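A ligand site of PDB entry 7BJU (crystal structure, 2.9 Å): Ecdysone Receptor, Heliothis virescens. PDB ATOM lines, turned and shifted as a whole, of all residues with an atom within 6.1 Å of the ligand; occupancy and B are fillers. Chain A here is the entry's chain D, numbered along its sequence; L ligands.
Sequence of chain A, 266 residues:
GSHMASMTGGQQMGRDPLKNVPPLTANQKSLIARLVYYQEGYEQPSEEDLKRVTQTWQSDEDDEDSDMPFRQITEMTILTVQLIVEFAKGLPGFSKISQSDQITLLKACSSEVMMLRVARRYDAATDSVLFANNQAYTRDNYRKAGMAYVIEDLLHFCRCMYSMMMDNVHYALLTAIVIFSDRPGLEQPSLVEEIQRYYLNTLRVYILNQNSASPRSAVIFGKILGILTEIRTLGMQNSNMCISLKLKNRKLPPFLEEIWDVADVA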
ATOM      1  N   PHE A  70     -22.758  -6.839 -25.593  1.00  0.00           N
ATOM      2  CA  PHE A  70     -22.462  -6.983 -24.179  1.00  0.00           C
ATOM      3  C   PHE A  70     -21.538  -8.172 -23.919  1.00  0.00           C
ATOM      4  O   PHE A  70     -20.822  -8.191 -22.917  1.00  0.00           O
ATOM      5  CB  PHE A  70     -23.749  -7.124 -23.376  1.00  0.00           C
ATOM      6  CG  PHE A  70     -23.546  -7.189 -21.892  1.00  0.00           C
ATOM      7  CD1 PHE A  70     -23.330  -6.030 -21.157  1.00  0.00           C
ATOM      8  CD2 PHE A  70     -23.575  -8.398 -21.224  1.00  0.00           C
ATOM      9  CE1 PHE A  70     -23.139  -6.081 -19.792  1.00  0.00           C
ATOM     10  CE2 PHE A  70     -23.388  -8.462 -19.853  1.00  0.00           C
ATOM     11  CZ  PHE A  70     -23.168  -7.297 -19.140  1.00  0.00           C
ATOM     12  N   ILE A  73     -17.800  -7.104 -24.595  1.00  0.00           N
ATOM     13  CA  ILE A  73     -17.244  -6.334 -23.498  1.00  0.00           C
ATOM     14  C   ILE A  73     -16.855  -7.257 -22.344  1.00  0.00           C
ATOM     15  O   ILE A  73     -15.751  -7.159 -21.799  1.00  0.00           O
ATOM     16  CB  ILE A  73     -18.244  -5.249 -23.041  1.00  0.00           C
ATOM     17  CG1 ILE A  73     -18.567  -4.288 -24.189  1.00  0.00           C
ATOM     18  CG2 ILE A  73     -17.708  -4.487 -21.837  1.00  0.00           C
ATOM     19  CD1 ILE A  73     -19.581  -3.236 -23.831  1.00  0.00           C
ATOM     20  N   THR A  74     -17.756  -8.160 -21.964  1.00  0.00           N
ATOM     21  CA  THR A  74     -17.487  -9.052 -20.844  1.00  0.00           C
ATOM     22  C   THR A  74     -16.351 -10.021 -21.150  1.00  0.00           C
ATOM     23  O   THR A  74     -15.587 -10.379 -20.251  1.00  0.00           O
ATOM     24  CB  THR A  74     -18.748  -9.830 -20.465  1.00  0.00           C
ATOM     25  OG1 THR A  74     -19.267 -10.502 -21.622  1.00  0.00           O
ATOM     26  CG2 THR A  74     -19.811  -8.876 -19.915  1.00  0.00           C
ATOM     27  N   THR A  77     -13.058  -8.000 -21.126  1.00  0.00           N
ATOM     28  CA  THR A  77     -12.729  -7.614 -19.756  1.00  0.00           C
ATOM     29  C   THR A  77     -12.130  -8.790 -18.980  1.00  0.00           C
ATOM     30  O   THR A  77     -11.148  -8.617 -18.254  1.00  0.00           O
ATOM     31  CB  THR A  77     -13.965  -7.071 -19.056  1.00  0.00           C
ATOM     32  OG1 THR A  77     -14.365  -5.844 -19.687  1.00  0.00           O
ATOM     33  CG2 THR A  77     -13.686  -6.802 -17.587  1.00  0.00           C
ATOM     34  N   SER A 110      -9.250  -4.251  -9.548  1.00  0.00           N
ATOM     35  CA  SER A 110      -9.485  -4.764 -10.897  1.00  0.00           C
ATOM     36  C   SER A 110     -10.165  -3.724 -11.779  1.00  0.00           C
ATOM     37  O   SER A 110      -9.717  -3.469 -12.905  1.00  0.00           O
ATOM     38  CB  SER A 110     -10.310  -6.045 -10.838  1.00  0.00           C
ATOM     39  OG  SER A 110     -11.499  -5.844 -10.087  1.00  0.00           O
ATOM     40  N   SER A 111     -11.234  -3.107 -11.291  1.00  0.00           N
ATOM     41  CA  SER A 111     -11.957  -2.138 -12.108  1.00  0.00           C
ATOM     42  C   SER A 111     -11.178  -0.829 -12.247  1.00  0.00           C
ATOM     43  O   SER A 111     -11.189  -0.199 -13.311  1.00  0.00           O
ATOM     44  CB  SER A 111     -13.344  -1.871 -11.530  1.00  0.00           C
ATOM     45  OG  SER A 111     -13.257  -1.167 -10.292  1.00  0.00           O
ATOM     46  N   MET A 114      -8.531  -1.306 -14.711  1.00  0.00           N
ATOM     47  CA  MET A 114      -9.155  -1.384 -16.029  1.00  0.00           C
ATOM     48  C   MET A 114      -9.370  -0.002 -16.618  1.00  0.00           C
ATOM     49  O   MET A 114      -9.256   0.189 -17.838  1.00  0.00           O
ATOM     50  CB  MET A 114     -10.468  -2.146 -15.947  1.00  0.00           C
ATOM     51  CG  MET A 114     -10.324  -3.666 -15.964  1.00  0.00           C
ATOM     52  SD  MET A 114     -10.893  -4.415 -17.495  1.00  0.00           S
ATOM     53  CE  MET A 114      -9.757  -3.681 -18.685  1.00  0.00           C
ATOM     54  N   MET A 115      -9.693   0.986 -15.774  1.00  0.00           N
ATOM     55  CA  MET A 115      -9.839   2.354 -16.259  1.00  0.00           C
ATOM     56  C   MET A 115      -8.503   2.898 -16.757  1.00  0.00           C
ATOM     57  O   MET A 115      -8.450   3.604 -17.769  1.00  0.00           O
ATOM     58  CB  MET A 115     -10.406   3.248 -15.159  1.00  0.00           C
ATOM     59  CG  MET A 115     -11.742   2.778 -14.605  1.00  0.00           C
ATOM     60  SD  MET A 115     -13.086   2.888 -15.797  1.00  0.00           S
ATOM     61  CE  MET A 115     -14.418   2.107 -14.881  1.00  0.00           C
ATOM     62  N   VAL A 118      -7.551   1.216 -20.233  1.00  0.00           N
ATOM     63  CA  VAL A 118      -8.339   1.774 -21.330  1.00  0.00           C
ATOM     64  C   VAL A 118      -7.945   3.218 -21.588  1.00  0.00           C
ATOM     65  O   VAL A 118      -7.833   3.643 -22.743  1.00  0.00           O
ATOM     66  CB  VAL A 118      -9.849   1.636 -21.026  1.00  0.00           C
ATOM     67  CG1 VAL A 118     -10.667   2.462 -22.008  1.00  0.00           C
ATOM     68  CG2 VAL A 118     -10.260   0.174 -21.081  1.00  0.00           C
ATOM     69  N   TYR A 137     -14.656  -1.862 -26.856  1.00  0.00           N
ATOM     70  CA  TYR A 137     -14.564  -0.616 -26.111  1.00  0.00           C
ATOM     71  C   TYR A 137     -14.774   0.624 -26.984  1.00  0.00           C
ATOM     72  O   TYR A 137     -14.415   1.727 -26.567  1.00  0.00           O
ATOM     73  CB  TYR A 137     -13.227  -0.539 -25.377  1.00  0.00           C
ATOM     74  CG  TYR A 137     -13.040  -1.644 -24.373  1.00  0.00           C
ATOM     75  CD1 TYR A 137     -14.131  -2.235 -23.751  1.00  0.00           C
ATOM     76  CD2 TYR A 137     -11.771  -2.111 -24.031  1.00  0.00           C
ATOM     77  CE1 TYR A 137     -13.980  -3.253 -22.829  1.00  0.00           C
ATOM     78  CE2 TYR A 137     -11.606  -3.126 -23.111  1.00  0.00           C
ATOM     79  CZ  TYR A 137     -12.707  -3.685 -22.515  1.00  0.00           C
ATOM     80  OH  TYR A 137     -12.543  -4.700 -21.595  1.00  0.00           O
ATOM     81  N   TYR A 142     -20.710   0.008 -27.013  1.00  0.00           N
ATOM     82  CA  TYR A 142     -21.294   0.449 -25.746  1.00  0.00           C
ATOM     83  C   TYR A 142     -22.692   0.998 -25.947  1.00  0.00           C
ATOM     84  O   TYR A 142     -23.552   0.840 -25.075  1.00  0.00           O
ATOM     85  CB  TYR A 142     -20.394   1.487 -25.090  1.00  0.00           C
ATOM     86  CG  TYR A 142     -19.419   0.914 -24.084  1.00  0.00           C
ATOM     87  CD1 TYR A 142     -18.250   0.282 -24.499  1.00  0.00           C
ATOM     88  CD2 TYR A 142     -19.673   1.005 -22.724  1.00  0.00           C
ATOM     89  CE1 TYR A 142     -17.364  -0.239 -23.583  1.00  0.00           C
ATOM     90  CE2 TYR A 142     -18.784   0.480 -21.799  1.00  0.00           C
ATOM     91  CZ  TYR A 142     -17.635  -0.141 -22.238  1.00  0.00           C
ATOM     92  OH  TYR A 142     -16.754  -0.661 -21.308  1.00  0.00           O
ATOM     93  N   MET A 147     -25.051   0.529 -22.519  1.00  0.00           N
ATOM     94  CA  MET A 147     -24.223   1.303 -21.607  1.00  0.00           C
ATOM     95  C   MET A 147     -23.570   2.474 -22.337  1.00  0.00           C
ATOM     96  O   MET A 147     -22.354   2.657 -22.280  1.00  0.00           O
ATOM     97  CB  MET A 147     -23.157   0.394 -20.961  1.00  0.00           C
ATOM     98  CG  MET A 147     -22.668  -0.727 -21.853  1.00  0.00           C
ATOM     99  SD  MET A 147     -21.979  -2.085 -20.897  1.00  0.00           S
ATOM    100  CE  MET A 147     -23.411  -2.565 -19.948  1.00  0.00           C
ATOM    101  N   VAL A 150     -22.263   5.832 -20.193  1.00  0.00           N
ATOM    102  CA  VAL A 150     -20.985   5.753 -19.488  1.00  0.00           C
ATOM    103  C   VAL A 150     -19.814   6.263 -20.331  1.00  0.00           C
ATOM    104  O   VAL A 150     -18.765   6.604 -19.773  1.00  0.00           O
ATOM    105  CB  VAL A 150     -20.787   4.294 -19.022  1.00  0.00           C
ATOM    106  CG1 VAL A 150     -19.427   3.732 -19.434  1.00  0.00           C
ATOM    107  CG2 VAL A 150     -21.010   4.188 -17.524  1.00  0.00           C
ATOM    108  N   ILE A 151     -20.004   6.377 -21.648  1.00  0.00           N
ATOM    109  CA  ILE A 151     -18.892   6.675 -22.551  1.00  0.00           C
ATOM    110  C   ILE A 151     -18.278   8.032 -22.229  1.00  0.00           C
ATOM    111  O   ILE A 151     -17.045   8.172 -22.166  1.00  0.00           O
ATOM    112  CB  ILE A 151     -19.373   6.611 -24.016  1.00  0.00           C
ATOM    113  CG1 ILE A 151     -19.969   5.247 -24.322  1.00  0.00           C
ATOM    114  CG2 ILE A 151     -18.237   6.935 -24.969  1.00  0.00           C
ATOM    115  CD1 ILE A 151     -20.667   5.158 -25.664  1.00  0.00           C
ATOM    116  N   ASP A 153     -18.284   9.878 -19.467  1.00  0.00           N
ATOM    117  CA  ASP A 153     -17.529   9.872 -18.219  1.00  0.00           C
ATOM    118  C   ASP A 153     -16.175   9.176 -18.399  1.00  0.00           C
ATOM    119  O   ASP A 153     -15.178   9.586 -17.800  1.00  0.00           O
ATOM    120  CB  ASP A 153     -18.329   9.186 -17.111  1.00  0.00           C
ATOM    121  CG  ASP A 153     -19.468  10.056 -16.601  1.00  0.00           C
ATOM    122  OD1 ASP A 153     -19.580  11.216 -17.037  1.00  0.00           O
ATOM    123  OD2 ASP A 153     -20.252   9.575 -15.757  1.00  0.00           O
ATOM    124  N   LEU A 154     -16.132   8.135 -19.237  1.00  0.00           N
ATOM    125  CA  LEU A 154     -14.876   7.438 -19.487  1.00  0.00           C
ATOM    126  C   LEU A 154     -13.926   8.311 -20.300  1.00  0.00           C
ATOM    127  O   LEU A 154     -12.761   8.480 -19.943  1.00  0.00           O
ATOM    128  CB  LEU A 154     -15.155   6.124 -20.213  1.00  0.00           C
ATOM    129  CG  LEU A 154     -13.909   5.320 -20.592  1.00  0.00           C
ATOM    130  CD1 LEU A 154     -13.178   4.861 -19.341  1.00  0.00           C
ATOM    131  CD2 LEU A 154     -14.279   4.137 -21.467  1.00  0.00           C
ATOM    132  N   THR A 233     -13.929   7.020  -8.043  1.00  0.00           N
ATOM    133  CA  THR A 233     -15.260   7.308  -8.568  1.00  0.00           C
ATOM    134  C   THR A 233     -15.617   6.358  -9.701  1.00  0.00           C
ATOM    135  O   THR A 233     -16.727   5.830  -9.759  1.00  0.00           O
ATOM    136  CB  THR A 233     -15.329   8.769  -9.041  1.00  0.00           C
ATOM    137  OG1 THR A 233     -14.985   9.642  -7.961  1.00  0.00           O
ATOM    138  CG2 THR A 233     -16.730   9.103  -9.532  1.00  0.00           C
ATOM    139  N   LEU A 234     -14.674   6.140 -10.623  1.00  0.00           N
ATOM    140  CA  LEU A 234     -14.935   5.246 -11.761  1.00  0.00           C
ATOM    141  C   LEU A 234     -15.201   3.821 -11.288  1.00  0.00           C
ATOM    142  O   LEU A 234     -16.097   3.148 -11.804  1.00  0.00           O
ATOM    143  CB  LEU A 234     -13.753   5.295 -12.731  1.00  0.00           C
ATOM    144  CG  LEU A 234     -13.352   6.675 -13.241  1.00  0.00           C
ATOM    145  CD1 LEU A 234     -12.205   6.556 -14.229  1.00  0.00           C
ATOM    146  CD2 LEU A 234     -14.535   7.389 -13.863  1.00  0.00           C
ATOM    147  N   GLN A 237     -18.702   3.824 -10.016  1.00  0.00           N
ATOM    148  CA  GLN A 237     -19.642   3.816 -11.142  1.00  0.00           C
ATOM    149  C   GLN A 237     -19.701   2.441 -11.793  1.00  0.00           C
ATOM    150  O   GLN A 237     -20.763   2.009 -12.258  1.00  0.00           O
ATOM    151  CB  GLN A 237     -19.247   4.877 -12.166  1.00  0.00           C
ATOM    152  CG  GLN A 237     -19.382   6.312 -11.680  1.00  0.00           C
ATOM    153  CD  GLN A 237     -19.049   7.322 -12.754  1.00  0.00           C
ATOM    154  OE1 GLN A 237     -17.884   7.508 -13.108  1.00  0.00           O
ATOM    155  NE2 GLN A 237     -20.065   7.995 -13.277  1.00  0.00           N
ATOM    156  N   ASN A 238     -18.562   1.738 -11.839  1.00  0.00           N
ATOM    157  CA  ASN A 238     -18.576   0.360 -12.326  1.00  0.00           C
ATOM    158  C   ASN A 238     -19.381  -0.540 -11.400  1.00  0.00           C
ATOM    159  O   ASN A 238     -20.136  -1.404 -11.862  1.00  0.00           O
ATOM    160  CB  ASN A 238     -17.147  -0.153 -12.477  1.00  0.00           C
ATOM    161  CG  ASN A 238     -17.099  -1.622 -12.856  1.00  0.00           C
ATOM    162  OD1 ASN A 238     -17.359  -1.985 -14.005  1.00  0.00           O
ATOM    163  ND2 ASN A 238     -16.767  -2.469 -11.892  1.00  0.00           N
ATOM    164  N   SER A 239     -19.231  -0.349 -10.085  1.00  0.00           N
ATOM    165  CA  SER A 239     -20.026  -1.133  -9.129  1.00  0.00           C
ATOM    166  C   SER A 239     -21.507  -0.809  -9.263  1.00  0.00           C
ATOM    167  O   SER A 239     -22.353  -1.705  -9.105  1.00  0.00           O
ATOM    168  CB  SER A 239     -19.541  -0.870  -7.705  1.00  0.00           C
ATOM    169  OG  SER A 239     -18.224  -1.348  -7.512  1.00  0.00           O
ATOM    170  N   MET A 241     -23.036  -0.015 -12.011  1.00  0.00           N
ATOM    171  CA  MET A 241     -23.567  -0.680 -13.196  1.00  0.00           C
ATOM    172  C   MET A 241     -23.806  -2.161 -12.927  1.00  0.00           C
ATOM    173  O   MET A 241     -24.819  -2.718 -13.383  1.00  0.00           O
ATOM    174  CB  MET A 241     -22.634  -0.492 -14.389  1.00  0.00           C
ATOM    175  CG  MET A 241     -23.098  -1.212 -15.647  1.00  0.00           C
ATOM    176  SD  MET A 241     -22.163  -0.759 -17.125  1.00  0.00           S
ATOM    177  CE  MET A 241     -22.658   0.944 -17.326  1.00  0.00           C
ATOM    178  N   CYS A 242     -22.904  -2.815 -12.199  1.00  0.00           N
ATOM    179  CA  CYS A 242     -23.124  -4.207 -11.813  1.00  0.00           C
ATOM    180  C   CYS A 242     -24.412  -4.355 -11.027  1.00  0.00           C
ATOM    181  O   CYS A 242     -25.149  -5.338 -11.207  1.00  0.00           O
ATOM    182  CB  CYS A 242     -21.933  -4.724 -11.007  1.00  0.00           C
ATOM    183  SG  CYS A 242     -20.373  -4.852 -11.916  1.00  0.00           S
ATOM    184  N   LEU A 245     -27.300  -4.027 -13.545  1.00  0.00           N
ATOM    185  CA  LEU A 245     -27.507  -5.219 -14.360  1.00  0.00           C
ATOM    186  C   LEU A 245     -28.311  -6.273 -13.606  1.00  0.00           C
ATOM    187  O   LEU A 245     -29.167  -6.942 -14.189  1.00  0.00           O
ATOM    188  CB  LEU A 245     -26.158  -5.787 -14.807  1.00  0.00           C
ATOM    189  CG  LEU A 245     -25.308  -4.862 -15.683  1.00  0.00           C
ATOM    190  CD1 LEU A 245     -23.963  -5.484 -15.972  1.00  0.00           C
ATOM    191  CD2 LEU A 245     -26.036  -4.523 -16.982  1.00  0.00           C
ATOM    192  N   LEU A 252     -23.688 -11.103 -15.437  1.00  0.00           N
ATOM    193  CA  LEU A 252     -22.269 -11.087 -15.789  1.00  0.00           C
ATOM    194  C   LEU A 252     -21.730 -12.510 -15.863  1.00  0.00           C
ATOM    195  O   LEU A 252     -22.258 -13.411 -15.197  1.00  0.00           O
ATOM    196  CB  LEU A 252     -21.477 -10.301 -14.755  1.00  0.00           C
ATOM    197  CG  LEU A 252     -20.773  -9.025 -15.224  1.00  0.00           C
ATOM    198  CD1 LEU A 252     -21.669  -8.240 -16.140  1.00  0.00           C
ATOM    199  CD2 LEU A 252     -20.355  -8.189 -14.030  1.00  0.00           C
ATOM    200  N   LEU A 256     -16.552 -12.464 -13.557  1.00  0.00           N
ATOM    201  CA  LEU A 256     -16.759 -11.068 -13.169  1.00  0.00           C
ATOM    202  C   LEU A 256     -17.689 -10.948 -11.976  1.00  0.00           C
ATOM    203  O   LEU A 256     -17.543 -10.029 -11.161  1.00  0.00           O
ATOM    204  CB  LEU A 256     -17.301 -10.275 -14.359  1.00  0.00           C
ATOM    205  CG  LEU A 256     -16.424 -10.238 -15.602  1.00  0.00           C
ATOM    206  CD1 LEU A 256     -17.059  -9.380 -16.683  1.00  0.00           C
ATOM    207  CD2 LEU A 256     -15.026  -9.755 -15.264  1.00  0.00           C
ATOM    208  N   TRP A 260     -16.329  -8.891  -8.764  1.00  0.00           N
ATOM    209  CA  TRP A 260     -17.011  -7.624  -8.531  1.00  0.00           C
ATOM    210  C   TRP A 260     -18.138  -7.763  -7.509  1.00  0.00           C
ATOM    211  O   TRP A 260     -18.997  -6.874  -7.427  1.00  0.00           O
ATOM    212  CB  TRP A 260     -17.500  -7.041  -9.856  1.00  0.00           C
ATOM    213  CG  TRP A 260     -16.370  -6.484 -10.662  1.00  0.00           C
ATOM    214  CD1 TRP A 260     -15.130  -6.144 -10.201  1.00  0.00           C
ATOM    215  CD2 TRP A 260     -16.348  -6.225 -12.079  1.00  0.00           C
ATOM    216  NE1 TRP A 260     -14.345  -5.680 -11.220  1.00  0.00           N
ATOM    217  CE2 TRP A 260     -15.065  -5.721 -12.386  1.00  0.00           C
ATOM    218  CE3 TRP A 260     -17.283  -6.367 -13.107  1.00  0.00           C
ATOM    219  CZ2 TRP A 260     -14.707  -5.354 -13.684  1.00  0.00           C
ATOM    220  CZ3 TRP A 260     -16.920  -6.010 -14.388  1.00  0.00           C
ATOM    221  CH2 TRP A 260     -15.641  -5.511 -14.673  1.00  0.00           C
HETATM  222  C1  LIG L   1     -14.529  -1.871 -19.451  1.00  0.00           C
HETATM  223  C2  LIG L   1     -13.488  -0.988 -19.690  1.00  0.00           C
HETATM  224  C3  LIG L   1     -12.859  -0.365 -18.650  1.00  0.00           C
HETATM  225  C4  LIG L   1     -13.248  -0.614 -17.346  1.00  0.00           C
HETATM  226  C5  LIG L   1     -14.279  -1.507 -17.104  1.00  0.00           C
HETATM  227  C6  LIG L   1     -14.944  -2.138 -18.151  1.00  0.00           C
HETATM  228  C7  LIG L   1     -16.105  -3.012 -17.924  1.00  0.00           C
HETATM  229 CL1  LIG L   1     -14.718  -1.815 -15.454  1.00  0.00          CL
HETATM  230  N1  LIG L   1     -16.160  -4.283 -18.279  1.00  0.00           N
HETATM  231  C8  LIG L   1     -17.411  -4.743 -17.943  1.00  0.00           C
HETATM  232  C9  LIG L   1     -18.149  -3.748 -17.357  1.00  0.00           C
HETATM  233  N2  LIG L   1     -17.293  -2.651 -17.353  1.00  0.00           N
HETATM  234  C10 LIG L   1     -17.803  -6.157 -18.212  1.00  0.00           C
HETATM  235  C11 LIG L   1     -19.560  -3.685 -16.831  1.00  0.00           C
HETATM  236  N3  LIG L   1     -17.632  -1.410 -16.833  1.00  0.00           N
HETATM  237  C12 LIG L   1     -17.895  -0.419 -17.718  1.00  0.00           C
HETATM  238  C13 LIG L   1     -19.774  -4.405 -15.526  1.00  0.00           C
HETATM  239  C14 LIG L   1     -20.630  -4.027 -17.857  1.00  0.00           C
HETATM  240  O1  LIG L   1     -18.064  -0.612 -18.911  1.00  0.00           O
HETATM  241  C15 LIG L   1     -17.964   0.956 -17.106  1.00  0.00           C
HETATM  242  C16 LIG L   1     -18.880   1.180 -16.081  1.00  0.00           C
HETATM  243  C17 LIG L   1     -18.970   2.409 -15.465  1.00  0.00           C
HETATM  244  C18 LIG L   1     -18.145   3.435 -15.897  1.00  0.00           C
HETATM  245  C19 LIG L   1     -17.231   3.215 -16.931  1.00  0.00           C
HETATM  246  C20 LIG L   1     -17.126   1.977 -17.556  1.00  0.00           C
HETATM  247  C21 LIG L   1     -16.121   1.761 -18.659  1.00  0.00           C
HETATM  248  O2  LIG L   1     -18.281   4.665 -15.292  1.00  0.00           O
HETATM  249  C22 LIG L   1     -17.721   5.737 -16.056  1.00  0.00           C
HETATM  250  C23 LIG L   1     -16.374   5.383 -16.568  1.00  0.00           C
HETATM  251  O3  LIG L   1     -16.414   4.220 -17.398  1.00  0.00           O
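OG1 of Thr 74 is in hydrogen-bond range of O of Phe 70.
SG of Cys 242 is in hydrogen-bond range of O of Asn 238, 3.5 Å away.
OG of Ser 110 is in hydrogen-bond range of NE1 of Trp 260 (3.1 Å).
The side-chain hydroxyl of Thr 77 is in hydrogen-bond range of the backbone carbonyl oxygen of Ile 73 (2.8 Å).
The side-chain carboxylate (OD2) of Asp 153 sits at hydrogen-bond distance from the side-chain amide nitrogen (NE2) of Gln 237.
OG1 of Thr 77 lies within hydrogen-bond range of OH of Tyr 137, 2.9 Å away.
The backbone NH (N) of Met 147 is in hydrogen-bond range of the backbone carbonyl oxygen (O) of Tyr 142 (3.0 Å).
Residues that only touch the ligand: Gln 237, Val 150, Trp 260, Met 114, Val 118, Leu 154, Leu 256, Met 115, Asp 153, Met 241, Cys 242, Tyr 137, Met 147, Phe 70, Thr 74, Leu 234 and Ile 73.
Hydrophobic or aromatic side chains that line the ligand: Phe 70, Ile 73, Met 114, Met 115, Val 118, Tyr 137, Tyr 142, Met 147, Val 150, Leu 154, Leu 234, Met 241, Leu 256 and Trp 260.
Of the 27 residues printed, 20 come within 4 Å of the ligand.
Along chain A the residues within 4 Å of the ligand span positions 70 to 260.
The nearest printed residue that does not touch the ligand is Leu 245 (4.1 Å).
The side-chain hydroxyl of Thr 77 lies within hydrogen-bond range of a nitrogen (N1) of the ligand.
The side-chain hydroxyl of Tyr 142 is in hydrogen-bond range of an oxygen (O1) of the ligand (2.7 Å).
OD1 of Asn 238 lies within hydrogen-bond range of N3 of the ligand (2.9 Å).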
